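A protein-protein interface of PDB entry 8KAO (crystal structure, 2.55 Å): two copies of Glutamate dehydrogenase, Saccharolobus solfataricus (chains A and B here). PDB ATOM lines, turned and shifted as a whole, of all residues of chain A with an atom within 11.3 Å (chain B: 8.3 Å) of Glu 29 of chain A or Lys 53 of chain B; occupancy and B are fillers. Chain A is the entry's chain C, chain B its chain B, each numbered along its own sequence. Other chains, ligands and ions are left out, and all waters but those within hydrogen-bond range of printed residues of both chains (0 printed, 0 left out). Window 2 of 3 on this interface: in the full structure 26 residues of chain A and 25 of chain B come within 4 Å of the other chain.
NE of Arg 48 of chain B lies within hydrogen-bond range of O of Gly 52 of chain B, at 3.2 Å.
The side-chain carboxylate of Asp 51 of chain B sits at hydrogen-bond distance from the backbone NH of Lys 53 of chain B.
The side-chain hydroxyl of Tyr 18 of chain A sits at hydrogen-bond distance from the side-chain carboxylate of Asp 32 of chain A.
O of Ser 28 of chain A lies close to OD1 of Asp 32 of chain A (2.7 Å).
N of Leu 418 of chain A is in hydrogen-bond range of O of Met 413 of chain A.
The side-chain amino group (NZ) of Lys 44 of chain B sits at hydrogen-bond distance from the backbone carbonyl oxygen (O) of Val 33 of chain A, at 2.8 Å.
The side-chain amino group of Lys 44 of chain B lies within hydrogen-bond range of the backbone carbonyl oxygen of Gln 36 of chain A (2.9 Å).
The chain-end carboxylate (O) of Leu 419 of chain A is in salt-bridge range of the guanidinium group (NH1) of Arg 48 of chain B, at 2.8 Å.
The side-chain amino group (NZ) of Lys 53 of chain B lies within salt-bridge range of the side-chain carboxylate (OE1) of Glu 29 of chain A.
Glu 29 of chain A touches just these residues of chain B: Lys 53 (3.4 Å) and Leu 54 (3.6 Å).
Of the printed residues of chain B, Gln 36 of chain A touches Lys 44 (2.9 Å).
Of chain A, only Leu 419 comes within 4 Å of Arg 48 of chain B.
No residue of chain A comes within 4 Å of Ser 49 of chain B.
No residue of chain A comes within 4 Å of Asp 51 of chain B.
Lys 53 of chain B touches just one residue of chain A: Glu 29.
Leu 54 of chain B touches just these residues of chain A: Glu 29 and Leu 419.
No residue of chain A comes within 4 Å of Arg 55 of chain B.
Of the printed residues of chain A, Thr 56 of chain B touches Asp 32 and Val 33.
The nearest residue of chain B that does not touch Glu 29 of chain A is Thr 56 of chain B (4.3 Å).
The nearest residue of chain A that does not touch Lys 53 of chain B is Asp 27 of chain A (6.5 Å).
Of the 13 printed residues of chain B, 6 touch a printed residue of chain A.
Printed residues of chain B that touch a printed residue of chain A: Lys 44, Gln 46, Arg 48, Lys 53, Leu 54 and Thr 56.
Hydrophobic or aromatic side chains of chain B within 4 Å of the printed part of chain A: Leu 54.
Of the 25 printed residues of chain A, 7 touch a printed residue of chain B.
Printed residues of chain A that touch a printed residue of chain B: Glu 29, Asp 32, Val 33, Gln 36, Pro 37, Leu 418 and Leu 419.
Hydrophobic or aromatic side chains of chain A within 4 Å of the printed part of chain B: Val 33.
Among the printed residues, 11 pairs touch across the chains.
Among the printed residues, Asp or Glu carboxylates within 4 Å of a Lys or Arg side-chain nitrogen of the other chain: Glu 29 of chain A with Lys 53 of chain B.
Among the printed residues, pairs that only touch across the chains: Val 33 of chain A with Gln 46 of chain B, Pro 37 of chain A with Lys 44 of chain B, Val 33 of chain A with Thr 56 of chain B, Glu 29 of chain A with Leu 54 of chain B, Leu 418 of chain A with Gln 46 of chain B, Asp 32 of chain A with Thr 56 of chain B and Leu 419 of chain A with Leu 54 of chain B.
No position is printed for both chains.
Of the 11 pairs that touch across the chains among the printed residues, none has its exchanged pair printed and touching as well.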
ATOM      1  N   VAL A  14      -0.306 -20.794  -0.842  1.00  0.00           N
ATOM      2  CA  VAL A  14      -0.503 -19.975  -2.025  1.00  0.00           C
ATOM      3  C   VAL A  14       0.678 -20.121  -2.995  1.00  0.00           C
ATOM      4  O   VAL A  14       0.431 -20.125  -4.192  1.00  0.00           O
ATOM      5  CB  VAL A  14      -0.733 -18.493  -1.672  1.00  0.00           C
ATOM      6  CG1 VAL A  14      -0.963 -17.670  -2.934  1.00  0.00           C
ATOM      7  CG2 VAL A  14      -1.878 -18.289  -0.688  1.00  0.00           C
ATOM      8  N   LEU A  17       0.443 -23.320  -4.839  1.00  0.00           N
ATOM      9  CA  LEU A  17      -0.614 -23.235  -5.832  1.00  0.00           C
ATOM     10  C   LEU A  17      -0.178 -22.464  -7.082  1.00  0.00           C
ATOM     11  O   LEU A  17      -0.601 -22.821  -8.182  1.00  0.00           O
ATOM     12  CB  LEU A  17      -1.835 -22.584  -5.185  1.00  0.00           C
ATOM     13  CG  LEU A  17      -3.015 -22.351  -6.118  1.00  0.00           C
ATOM     14  CD1 LEU A  17      -3.586 -23.680  -6.568  1.00  0.00           C
ATOM     15  CD2 LEU A  17      -4.072 -21.474  -5.446  1.00  0.00           C
ATOM     16  N   TYR A  18       0.617 -21.388  -6.941  1.00  0.00           N
ATOM     17  CA  TYR A  18       1.093 -20.649  -8.114  1.00  0.00           C
ATOM     18  C   TYR A  18       2.097 -21.502  -8.878  1.00  0.00           C
ATOM     19  O   TYR A  18       2.025 -21.607 -10.094  1.00  0.00           O
ATOM     20  CB  TYR A  18       1.689 -19.282  -7.764  1.00  0.00           C
ATOM     21  CG  TYR A  18       0.642 -18.210  -7.613  1.00  0.00           C
ATOM     22  CD1 TYR A  18      -0.383 -18.360  -6.693  1.00  0.00           C
ATOM     23  CD2 TYR A  18       0.634 -17.076  -8.415  1.00  0.00           C
ATOM     24  CE1 TYR A  18      -1.376 -17.408  -6.548  1.00  0.00           C
ATOM     25  CE2 TYR A  18      -0.362 -16.113  -8.287  1.00  0.00           C
ATOM     26  CZ  TYR A  18      -1.373 -16.280  -7.351  1.00  0.00           C
ATOM     27  OH  TYR A  18      -2.397 -15.373  -7.169  1.00  0.00           O
ATOM     28  N   GLY A  21      -0.037 -23.799 -10.781  1.00  0.00           N
ATOM     29  CA  GLY A  21      -0.869 -23.043 -11.706  1.00  0.00           C
ATOM     30  C   GLY A  21      -0.127 -22.673 -12.993  1.00  0.00           C
ATOM     31  O   GLY A  21      -0.652 -22.846 -14.097  1.00  0.00           O
ATOM     32  N   GLU A  22       1.099 -22.163 -12.849  1.00  0.00           N
ATOM     33  CA  GLU A  22       1.881 -21.719 -13.992  1.00  0.00           C
ATOM     34  C   GLU A  22       2.228 -22.931 -14.837  1.00  0.00           C
ATOM     35  O   GLU A  22       2.009 -22.912 -16.049  1.00  0.00           O
ATOM     36  CB  GLU A  22       3.097 -20.933 -13.519  1.00  0.00           C
ATOM     37  CG  GLU A  22       2.695 -19.591 -12.930  1.00  0.00           C
ATOM     38  CD  GLU A  22       3.666 -19.033 -11.909  1.00  0.00           C
ATOM     39  OE1 GLU A  22       3.297 -18.051 -11.223  1.00  0.00           O
ATOM     40  OE2 GLU A  22       4.782 -19.593 -11.801  1.00  0.00           O
ATOM     41  N   GLY A  25      -0.622 -23.747 -16.950  1.00  0.00           N
ATOM     42  CA  GLY A  25      -0.986 -22.744 -17.938  1.00  0.00           C
ATOM     43  C   GLY A  25      -2.242 -21.954 -17.561  1.00  0.00           C
ATOM     44  O   GLY A  25      -3.005 -21.574 -18.441  1.00  0.00           O
ATOM     45  N   LEU A  26      -2.446 -21.671 -16.265  1.00  0.00           N
ATOM     46  CA  LEU A  26      -3.613 -20.914 -15.823  1.00  0.00           C
ATOM     47  C   LEU A  26      -3.244 -19.438 -15.716  1.00  0.00           C
ATOM     48  O   LEU A  26      -2.154 -19.102 -15.277  1.00  0.00           O
ATOM     49  CB  LEU A  26      -4.108 -21.437 -14.467  1.00  0.00           C
ATOM     50  CG  LEU A  26      -4.548 -22.903 -14.407  1.00  0.00           C
ATOM     51  CD1 LEU A  26      -4.963 -23.284 -12.990  1.00  0.00           C
ATOM     52  CD2 LEU A  26      -5.697 -23.195 -15.366  1.00  0.00           C
ATOM     53  N   ASP A  27      -4.174 -18.556 -16.113  1.00  0.00           N
ATOM     54  CA  ASP A  27      -3.985 -17.125 -15.940  1.00  0.00           C
ATOM     55  C   ASP A  27      -3.828 -16.875 -14.448  1.00  0.00           C
ATOM     56  O   ASP A  27      -4.443 -17.572 -13.643  1.00  0.00           O
ATOM     57  CB  ASP A  27      -5.172 -16.261 -16.391  1.00  0.00           C
ATOM     58  CG  ASP A  27      -6.114 -16.866 -17.418  1.00  0.00           C
ATOM     59  OD1 ASP A  27      -5.979 -18.071 -17.717  1.00  0.00           O
ATOM     60  OD2 ASP A  27      -7.008 -16.129 -17.888  1.00  0.00           O
ATOM     61  N   SER A  28      -3.075 -15.836 -14.090  1.00  0.00           N
ATOM     62  CA  SER A  28      -2.974 -15.431 -12.700  1.00  0.00           C
ATOM     63  C   SER A  28      -4.333 -14.994 -12.147  1.00  0.00           C
ATOM     64  O   SER A  28      -4.504 -14.944 -10.928  1.00  0.00           O
ATOM     65  CB  SER A  28      -1.949 -14.350 -12.531  1.00  0.00           C
ATOM     66  OG  SER A  28      -2.310 -13.219 -13.299  1.00  0.00           O
ATOM     67  N   GLU A  29      -5.286 -14.660 -13.033  1.00  0.00           N
ATOM     68  CA  GLU A  29      -6.630 -14.277 -12.609  1.00  0.00           C
ATOM     69  C   GLU A  29      -7.386 -15.506 -12.100  1.00  0.00           C
ATOM     70  O   GLU A  29      -8.122 -15.410 -11.120  1.00  0.00           O
ATOM     71  CB  GLU A  29      -7.443 -13.619 -13.732  1.00  0.00           C
ATOM     72  CG  GLU A  29      -6.749 -12.467 -14.457  1.00  0.00           C
ATOM     73  CD  GLU A  29      -6.052 -12.866 -15.747  1.00  0.00           C
ATOM     74  OE1 GLU A  29      -4.886 -12.483 -15.934  1.00  0.00           O
ATOM     75  OE2 GLU A  29      -6.677 -13.578 -16.557  1.00  0.00           O
ATOM     76  N   THR A  30      -7.205 -16.634 -12.803  1.00  0.00           N
ATOM     77  CA  THR A  30      -7.773 -17.922 -12.443  1.00  0.00           C
ATOM     78  C   THR A  30      -7.181 -18.398 -11.119  1.00  0.00           C
ATOM     79  O   THR A  30      -7.895 -18.806 -10.207  1.00  0.00           O
ATOM     80  CB  THR A  30      -7.538 -18.950 -13.563  1.00  0.00           C
ATOM     81  OG1 THR A  30      -8.328 -18.582 -14.691  1.00  0.00           O
ATOM     82  CG2 THR A  30      -7.921 -20.368 -13.203  1.00  0.00           C
ATOM     83  N   ILE A  31      -5.858 -18.374 -11.024  1.00  0.00           N
ATOM     84  CA  ILE A  31      -5.195 -18.793  -9.804  1.00  0.00           C
ATOM     85  C   ILE A  31      -5.651 -17.894  -8.654  1.00  0.00           C
ATOM     86  O   ILE A  31      -5.870 -18.408  -7.567  1.00  0.00           O
ATOM     87  CB  ILE A  31      -3.666 -18.810  -9.965  1.00  0.00           C
ATOM     88  CG1 ILE A  31      -3.203 -19.661 -11.150  1.00  0.00           C
ATOM     89  CG2 ILE A  31      -3.018 -19.295  -8.686  1.00  0.00           C
ATOM     90  CD1 ILE A  31      -1.747 -19.421 -11.532  1.00  0.00           C
ATOM     91  N   ASP A  32      -5.834 -16.585  -8.888  1.00  0.00           N
ATOM     92  CA  ASP A  32      -6.397 -15.683  -7.881  1.00  0.00           C
ATOM     93  C   ASP A  32      -7.731 -16.192  -7.329  1.00  0.00           C
ATOM     94  O   ASP A  32      -7.977 -16.134  -6.122  1.00  0.00           O
ATOM     95  CB  ASP A  32      -6.641 -14.270  -8.418  1.00  0.00           C
ATOM     96  CG  ASP A  32      -5.368 -13.465  -8.608  1.00  0.00           C
ATOM     97  OD1 ASP A  32      -4.275 -14.043  -8.424  1.00  0.00           O
ATOM     98  OD2 ASP A  32      -5.477 -12.266  -8.934  1.00  0.00           O
ATOM     99  N   VAL A  33      -8.606 -16.657  -8.226  1.00  0.00           N
ATOM    100  CA  VAL A  33      -9.898 -17.187  -7.833  1.00  0.00           C
ATOM    101  C   VAL A  33      -9.707 -18.458  -7.006  1.00  0.00           C
ATOM    102  O   VAL A  33     -10.278 -18.579  -5.923  1.00  0.00           O
ATOM    103  CB  VAL A  33     -10.780 -17.468  -9.063  1.00  0.00           C
ATOM    104  CG1 VAL A  33     -12.092 -18.123  -8.655  1.00  0.00           C
ATOM    105  CG2 VAL A  33     -11.040 -16.215  -9.884  1.00  0.00           C
ATOM    106  N   LEU A  34      -8.930 -19.417  -7.529  1.00  0.00           N
ATOM    107  CA  LEU A  34      -8.648 -20.644  -6.805  1.00  0.00           C
ATOM    108  C   LEU A  34      -8.051 -20.332  -5.436  1.00  0.00           C
ATOM    109  O   LEU A  34      -8.422 -20.930  -4.422  1.00  0.00           O
ATOM    110  CB  LEU A  34      -7.676 -21.495  -7.615  1.00  0.00           C
ATOM    111  CG  LEU A  34      -8.220 -22.062  -8.925  1.00  0.00           C
ATOM    112  CD1 LEU A  34      -7.165 -22.921  -9.615  1.00  0.00           C
ATOM    113  CD2 LEU A  34      -9.487 -22.866  -8.678  1.00  0.00           C
ATOM    114  N   SER A  35      -7.116 -19.391  -5.404  1.00  0.00           N
ATOM    115  CA  SER A  35      -6.384 -19.107  -4.180  1.00  0.00           C
ATOM    116  C   SER A  35      -7.322 -18.729  -3.021  1.00  0.00           C
ATOM    117  O   SER A  35      -7.135 -19.164  -1.892  1.00  0.00           O
ATOM    118  CB  SER A  35      -5.354 -18.034  -4.439  1.00  0.00           C
ATOM    119  OG  SER A  35      -4.503 -17.882  -3.308  1.00  0.00           O
ATOM    120  N   GLN A  36      -8.345 -17.916  -3.290  1.00  0.00           N
ATOM    121  CA  GLN A  36      -9.070 -17.259  -2.220  1.00  0.00           C
ATOM    122  C   GLN A  36     -10.228 -18.152  -1.798  1.00  0.00           C
ATOM    123  O   GLN A  36     -10.847 -18.822  -2.633  1.00  0.00           O
ATOM    124  CB  GLN A  36      -9.619 -15.894  -2.640  1.00  0.00           C
ATOM    125  CG  GLN A  36      -8.635 -15.029  -3.411  1.00  0.00           C
ATOM    126  CD  GLN A  36      -7.826 -14.156  -2.495  1.00  0.00           C
ATOM    127  OE1 GLN A  36      -8.324 -13.187  -1.931  1.00  0.00           O
ATOM    128  NE2 GLN A  36      -6.559 -14.506  -2.350  1.00  0.00           N
ATOM    129  N   PRO A  37     -10.575 -18.137  -0.494  1.00  0.00           N
ATOM    130  CA  PRO A  37     -11.708 -18.910   0.009  1.00  0.00           C
ATOM    131  C   PRO A  37     -12.989 -18.207  -0.424  1.00  0.00           C
ATOM    132  O   PRO A  37     -13.023 -16.977  -0.464  1.00  0.00           O
ATOM    133  CB  PRO A  37     -11.494 -18.872   1.529  1.00  0.00           C
ATOM    134  CG  PRO A  37     -10.862 -17.511   1.755  1.00  0.00           C
ATOM    135  CD  PRO A  37      -9.949 -17.316   0.558  1.00  0.00           C
ATOM    136  N   ASN A  65     -13.611 -23.639  -1.124  1.00  0.00           N
ATOM    137  CA  ASN A  65     -14.041 -23.929  -2.473  1.00  0.00           C
ATOM    138  C   ASN A  65     -15.120 -25.009  -2.451  1.00  0.00           C
ATOM    139  O   ASN A  65     -14.970 -26.000  -1.737  1.00  0.00           O
ATOM    140  CB  ASN A  65     -12.831 -24.363  -3.294  1.00  0.00           C
ATOM    141  CG  ASN A  65     -13.198 -24.471  -4.748  1.00  0.00           C
ATOM    142  OD1 ASN A  65     -13.894 -25.424  -5.121  1.00  0.00           O
ATOM    143  ND2 ASN A  65     -12.803 -23.464  -5.520  1.00  0.00           N
ATOM    144  N   VAL A 406      -6.160 -29.756  -8.955  1.00  0.00           N
ATOM    145  CA  VAL A 406      -6.521 -28.402  -9.360  1.00  0.00           C
ATOM    146  C   VAL A 406      -7.319 -28.421 -10.664  1.00  0.00           C
ATOM    147  O   VAL A 406      -8.084 -27.492 -10.948  1.00  0.00           O
ATOM    148  CB  VAL A 406      -5.278 -27.514  -9.540  1.00  0.00           C
ATOM    149  CG1 VAL A 406      -5.668 -26.149 -10.070  1.00  0.00           C
ATOM    150  CG2 VAL A 406      -4.477 -27.369  -8.264  1.00  0.00           C
ATOM    151  N   VAL A 410     -11.004 -26.764 -11.493  1.00  0.00           N
ATOM    152  CA  VAL A 410     -11.213 -25.788 -12.555  1.00  0.00           C
ATOM    153  C   VAL A 410     -12.192 -26.336 -13.613  1.00  0.00           C
ATOM    154  O   VAL A 410     -13.099 -25.627 -14.062  1.00  0.00           O
ATOM    155  CB  VAL A 410      -9.873 -25.321 -13.158  1.00  0.00           C
ATOM    156  CG1 VAL A 410      -9.084 -26.462 -13.764  1.00  0.00           C
ATOM    157  CG2 VAL A 410     -10.064 -24.242 -14.210  1.00  0.00           C
ATOM    158  N   MET A 413     -15.557 -25.886 -12.120  1.00  0.00           N
ATOM    159  CA  MET A 413     -15.941 -24.488 -12.069  1.00  0.00           C
ATOM    160  C   MET A 413     -16.356 -24.029 -13.472  1.00  0.00           C
ATOM    161  O   MET A 413     -17.327 -23.281 -13.621  1.00  0.00           O
ATOM    162  CB  MET A 413     -14.798 -23.638 -11.496  1.00  0.00           C
ATOM    163  CG  MET A 413     -14.632 -23.862 -10.005  1.00  0.00           C
ATOM    164  SD  MET A 413     -13.434 -22.809  -9.146  1.00  0.00           S
ATOM    165  CE  MET A 413     -14.297 -21.243  -8.995  1.00  0.00           C
ATOM    166  N   LYS A 414     -15.655 -24.511 -14.512  1.00  0.00           N
ATOM    167  CA  LYS A 414     -15.977 -24.133 -15.887  1.00  0.00           C
ATOM    168  C   LYS A 414     -17.425 -24.502 -16.191  1.00  0.00           C
ATOM    169  O   LYS A 414     -18.210 -23.647 -16.578  1.00  0.00           O
ATOM    170  CB  LYS A 414     -15.021 -24.786 -16.890  1.00  0.00           C
ATOM    171  CG  LYS A 414     -13.702 -24.038 -17.097  1.00  0.00           C
ATOM    172  CD  LYS A 414     -12.704 -24.801 -17.976  1.00  0.00           C
ATOM    173  CE  LYS A 414     -12.071 -23.941 -19.058  1.00  0.00           C
ATOM    174  NZ  LYS A 414     -11.143 -22.928 -18.487  1.00  0.00           N
ATOM    175  N   LEU A 418     -18.425 -20.708 -13.437  1.00  0.00           N
ATOM    176  CA  LEU A 418     -17.849 -19.902 -12.372  1.00  0.00           C
ATOM    177  C   LEU A 418     -16.471 -19.377 -12.773  1.00  0.00           C
ATOM    178  O   LEU A 418     -15.852 -18.635 -12.011  1.00  0.00           O
ATOM    179  CB  LEU A 418     -17.742 -20.774 -11.118  1.00  0.00           C
ATOM    180  CG  LEU A 418     -19.068 -21.265 -10.548  1.00  0.00           C
ATOM    181  CD1 LEU A 418     -18.823 -22.310  -9.466  1.00  0.00           C
ATOM    182  CD2 LEU A 418     -19.892 -20.087 -10.022  1.00  0.00           C
ATOM    183  N   LEU A 419     -16.010 -19.751 -13.973  1.00  0.00           N
ATOM    184  CA  LEU A 419     -14.634 -19.510 -14.377  1.00  0.00           C
ATOM    185  C   LEU A 419     -14.524 -19.412 -15.902  1.00  0.00           C
ATOM    186  O   LEU A 419     -13.848 -18.472 -16.363  1.00  0.00           O
ATOM    187  CB  LEU A 419     -13.806 -20.684 -13.856  1.00  0.00           C
ATOM    188  CG  LEU A 419     -12.390 -20.372 -13.399  1.00  0.00           C
ATOM    189  CD1 LEU A 419     -12.381 -19.264 -12.364  1.00  0.00           C
ATOM    190  CD2 LEU A 419     -11.780 -21.624 -12.815  1.00  0.00           C
ATOM    191  OXT LEU A 419     -15.087 -20.299 -16.564  1.00  0.00           O
ATOM    192  N   LYS B  44     -15.504 -13.959  -1.527  1.00  0.00           N
ATOM    193  CA  LYS B  44     -14.767 -13.744  -2.758  1.00  0.00           C
ATOM    194  C   LYS B  44     -15.770 -13.557  -3.893  1.00  0.00           C
ATOM    195  O   LYS B  44     -16.576 -14.439  -4.170  1.00  0.00           O
ATOM    196  CB  LYS B  44     -13.873 -14.955  -3.038  1.00  0.00           C
ATOM    197  CG  LYS B  44     -13.218 -14.979  -4.413  1.00  0.00           C
ATOM    198  CD  LYS B  44     -12.615 -16.315  -4.806  1.00  0.00           C
ATOM    199  CE  LYS B  44     -13.454 -17.496  -4.391  1.00  0.00           C
ATOM    200  NZ  LYS B  44     -12.812 -18.756  -4.824  1.00  0.00           N
ATOM    201  N   GLN B  46     -16.061 -13.047  -7.869  1.00  0.00           N
ATOM    202  CA  GLN B  46     -15.494 -12.955  -9.211  1.00  0.00           C
ATOM    203  C   GLN B  46     -16.481 -12.237 -10.138  1.00  0.00           C
ATOM    204  O   GLN B  46     -17.650 -12.612 -10.232  1.00  0.00           O
ATOM    205  CB  GLN B  46     -14.996 -14.291  -9.787  1.00  0.00           C
ATOM    206  CG  GLN B  46     -15.937 -15.482  -9.664  1.00  0.00           C
ATOM    207  CD  GLN B  46     -15.554 -16.429  -8.551  1.00  0.00           C
ATOM    208  OE1 GLN B  46     -14.665 -16.143  -7.745  1.00  0.00           O
ATOM    209  NE2 GLN B  46     -16.231 -17.570  -8.514  1.00  0.00           N
ATOM    210  N   ILE B  47     -15.966 -11.168 -10.765  1.00  0.00           N
ATOM    211  CA  ILE B  47     -16.637 -10.300 -11.722  1.00  0.00           C
ATOM    212  C   ILE B  47     -15.959 -10.485 -13.081  1.00  0.00           C
ATOM    213  O   ILE B  47     -14.724 -10.535 -13.173  1.00  0.00           O
ATOM    214  CB  ILE B  47     -16.541  -8.827 -11.251  1.00  0.00           C
ATOM    215  CG1 ILE B  47     -17.448  -8.548 -10.051  1.00  0.00           C
ATOM    216  CG2 ILE B  47     -16.802  -7.832 -12.375  1.00  0.00           C
ATOM    217  CD1 ILE B  47     -18.923  -8.609 -10.356  1.00  0.00           C
ATOM    218  N   ARG B  48     -16.774 -10.561 -14.138  1.00  0.00           N
ATOM    219  CA  ARG B  48     -16.248 -10.694 -15.487  1.00  0.00           C
ATOM    220  C   ARG B  48     -16.543  -9.418 -16.273  1.00  0.00           C
ATOM    221  O   ARG B  48     -17.655  -8.894 -16.251  1.00  0.00           O
ATOM    222  CB  ARG B  48     -16.805 -11.933 -16.194  1.00  0.00           C
ATOM    223  CG  ARG B  48     -15.921 -12.391 -17.345  1.00  0.00           C
ATOM    224  CD  ARG B  48     -16.157 -13.819 -17.794  1.00  0.00           C
ATOM    225  NE  ARG B  48     -14.859 -14.451 -17.970  1.00  0.00           N
ATOM    226  CZ  ARG B  48     -14.386 -15.398 -17.169  1.00  0.00           C
ATOM    227  NH1 ARG B  48     -15.187 -15.964 -16.280  1.00  0.00           N
ATOM    228  NH2 ARG B  48     -13.123 -15.785 -17.265  1.00  0.00           N
ATOM    229  N   SER B  49     -15.518  -8.936 -16.980  1.00  0.00           N
ATOM    230  CA  SER B  49     -15.618  -7.694 -17.719  1.00  0.00           C
ATOM    231  C   SER B  49     -16.166  -7.959 -19.121  1.00  0.00           C
ATOM    232  O   SER B  49     -16.371  -9.110 -19.521  1.00  0.00           O
ATOM    233  CB  SER B  49     -14.285  -7.016 -17.738  1.00  0.00           C
ATOM    234  OG  SER B  49     -14.457  -5.625 -17.928  1.00  0.00           O
ATOM    235  N   SER B  50     -16.435  -6.874 -19.855  1.00  0.00           N
ATOM    236  CA  SER B  50     -16.928  -6.982 -21.220  1.00  0.00           C
ATOM    237  C   SER B  50     -15.937  -7.724 -22.116  1.00  0.00           C
ATOM    238  O   SER B  50     -16.335  -8.533 -22.953  1.00  0.00           O
ATOM    239  CB  SER B  50     -17.246  -5.632 -21.779  1.00  0.00           C
ATOM    240  OG  SER B  50     -18.628  -5.374 -21.603  1.00  0.00           O
ATOM    241  N   ASP B  51     -14.646  -7.438 -21.911  1.00  0.00           N
ATOM    242  CA  ASP B  51     -13.572  -7.983 -22.729  1.00  0.00           C
ATOM    243  C   ASP B  51     -13.278  -9.437 -22.348  1.00  0.00           C
ATOM    244  O   ASP B  51     -12.408 -10.058 -22.952  1.00  0.00           O
ATOM    245  CB  ASP B  51     -12.330  -7.078 -22.641  1.00  0.00           C
ATOM    246  CG  ASP B  51     -11.936  -6.666 -21.228  1.00  0.00           C
ATOM    247  OD1 ASP B  51     -12.511  -7.222 -20.275  1.00  0.00           O
ATOM    248  OD2 ASP B  51     -11.075  -5.775 -21.087  1.00  0.00           O
ATOM    249  N   GLY B  52     -13.997  -9.984 -21.354  1.00  0.00           N
ATOM    250  CA  GLY B  52     -13.734 -11.319 -20.839  1.00  0.00           C
ATOM    251  C   GLY B  52     -12.780 -11.343 -19.636  1.00  0.00           C
ATOM    252  O   GLY B  52     -12.611 -12.396 -19.017  1.00  0.00           O
ATOM    253  N   LYS B  53     -12.168 -10.187 -19.308  1.00  0.00           N
ATOM    254  CA  LYS B  53     -11.234 -10.072 -18.194  1.00  0.00           C
ATOM    255  C   LYS B  53     -11.924 -10.470 -16.893  1.00  0.00           C
ATOM    256  O   LYS B  53     -13.045 -10.035 -16.628  1.00  0.00           O
ATOM    257  CB  LYS B  53     -10.699  -8.644 -18.017  1.00  0.00           C
ATOM    258  CG  LYS B  53      -9.553  -8.238 -18.938  1.00  0.00           C
ATOM    259  CD  LYS B  53      -8.259  -9.019 -18.737  1.00  0.00           C
ATOM    260  CE  LYS B  53      -7.646  -8.862 -17.352  1.00  0.00           C
ATOM    261  NZ  LYS B  53      -6.406  -9.666 -17.210  1.00  0.00           N
ATOM    262  N   LEU B  54     -11.222 -11.276 -16.087  1.00  0.00           N
ATOM    263  CA  LEU B  54     -11.713 -11.728 -14.796  1.00  0.00           C
ATOM    264  C   LEU B  54     -11.008 -10.926 -13.698  1.00  0.00           C
ATOM    265  O   LEU B  54      -9.800 -10.662 -13.745  1.00  0.00           O
ATOM    266  CB  LEU B  54     -11.450 -13.235 -14.674  1.00  0.00           C
ATOM    267  CG  LEU B  54     -12.653 -14.113 -14.323  1.00  0.00           C
ATOM    268  CD1 LEU B  54     -12.224 -15.570 -14.193  1.00  0.00           C
ATOM    269  CD2 LEU B  54     -13.349 -13.645 -13.049  1.00  0.00           C
ATOM    270  N   ARG B  55     -11.797 -10.468 -12.729  1.00  0.00           N
ATOM    271  CA  ARG B  55     -11.255  -9.793 -11.565  1.00  0.00           C
ATOM    272  C   ARG B  55     -12.010 -10.326 -10.359  1.00  0.00           C
ATOM    273  O   ARG B  55     -13.222 -10.490 -10.424  1.00  0.00           O
ATOM    274  CB  ARG B  55     -11.395  -8.274 -11.691  1.00  0.00           C
ATOM    275  CG  ARG B  55     -10.479  -7.645 -12.730  1.00  0.00           C
ATOM    276  CD  ARG B  55     -10.791  -6.167 -12.903  1.00  0.00           C
ATOM    277  NE  ARG B  55     -12.045  -5.954 -13.621  1.00  0.00           N
ATOM    278  CZ  ARG B  55     -12.705  -4.802 -13.646  1.00  0.00           C
ATOM    279  NH1 ARG B  55     -12.297  -3.776 -12.906  1.00  0.00           N
ATOM    280  NH2 ARG B  55     -13.788  -4.691 -14.400  1.00  0.00           N
ATOM    281  N   THR B  56     -11.292 -10.630  -9.279  1.00  0.00           N
ATOM    282  CA  THR B  56     -11.964 -11.045  -8.065  1.00  0.00           C
ATOM    283  C   THR B  56     -11.799  -9.924  -7.034  1.00  0.00           C
ATOM    284  O   THR B  56     -10.814  -9.201  -7.056  1.00  0.00           O
ATOM    285  CB  THR B  56     -11.598 -12.504  -7.729  1.00  0.00           C
ATOM    286  OG1 THR B  56     -11.434 -12.625  -6.316  1.00  0.00           O
ATOM    287  CG2 THR B  56     -10.355 -13.008  -8.416  1.00  0.00           C
ATOM    288  N   GLU B 122     -21.095  -4.154 -14.015  1.00  0.00           N
ATOM    289  CA  GLU B 122     -20.173  -4.872 -13.155  1.00  0.00           C
ATOM    290  C   GLU B 122     -20.499  -4.571 -11.704  1.00  0.00           C
ATOM    291  O   GLU B 122     -20.470  -5.465 -10.872  1.00  0.00           O
ATOM    292  CB  GLU B 122     -18.735  -4.481 -13.482  1.00  0.00           C
ATOM    293  CG  GLU B 122     -18.255  -5.057 -14.802  1.00  0.00           C
ATOM    294  CD  GLU B 122     -16.886  -4.569 -15.235  1.00  0.00           C
ATOM    295  OE1 GLU B 122     -16.636  -3.340 -15.154  1.00  0.00           O
ATOM    296  OE2 GLU B 122     -16.083  -5.413 -15.670  1.00  0.00           O
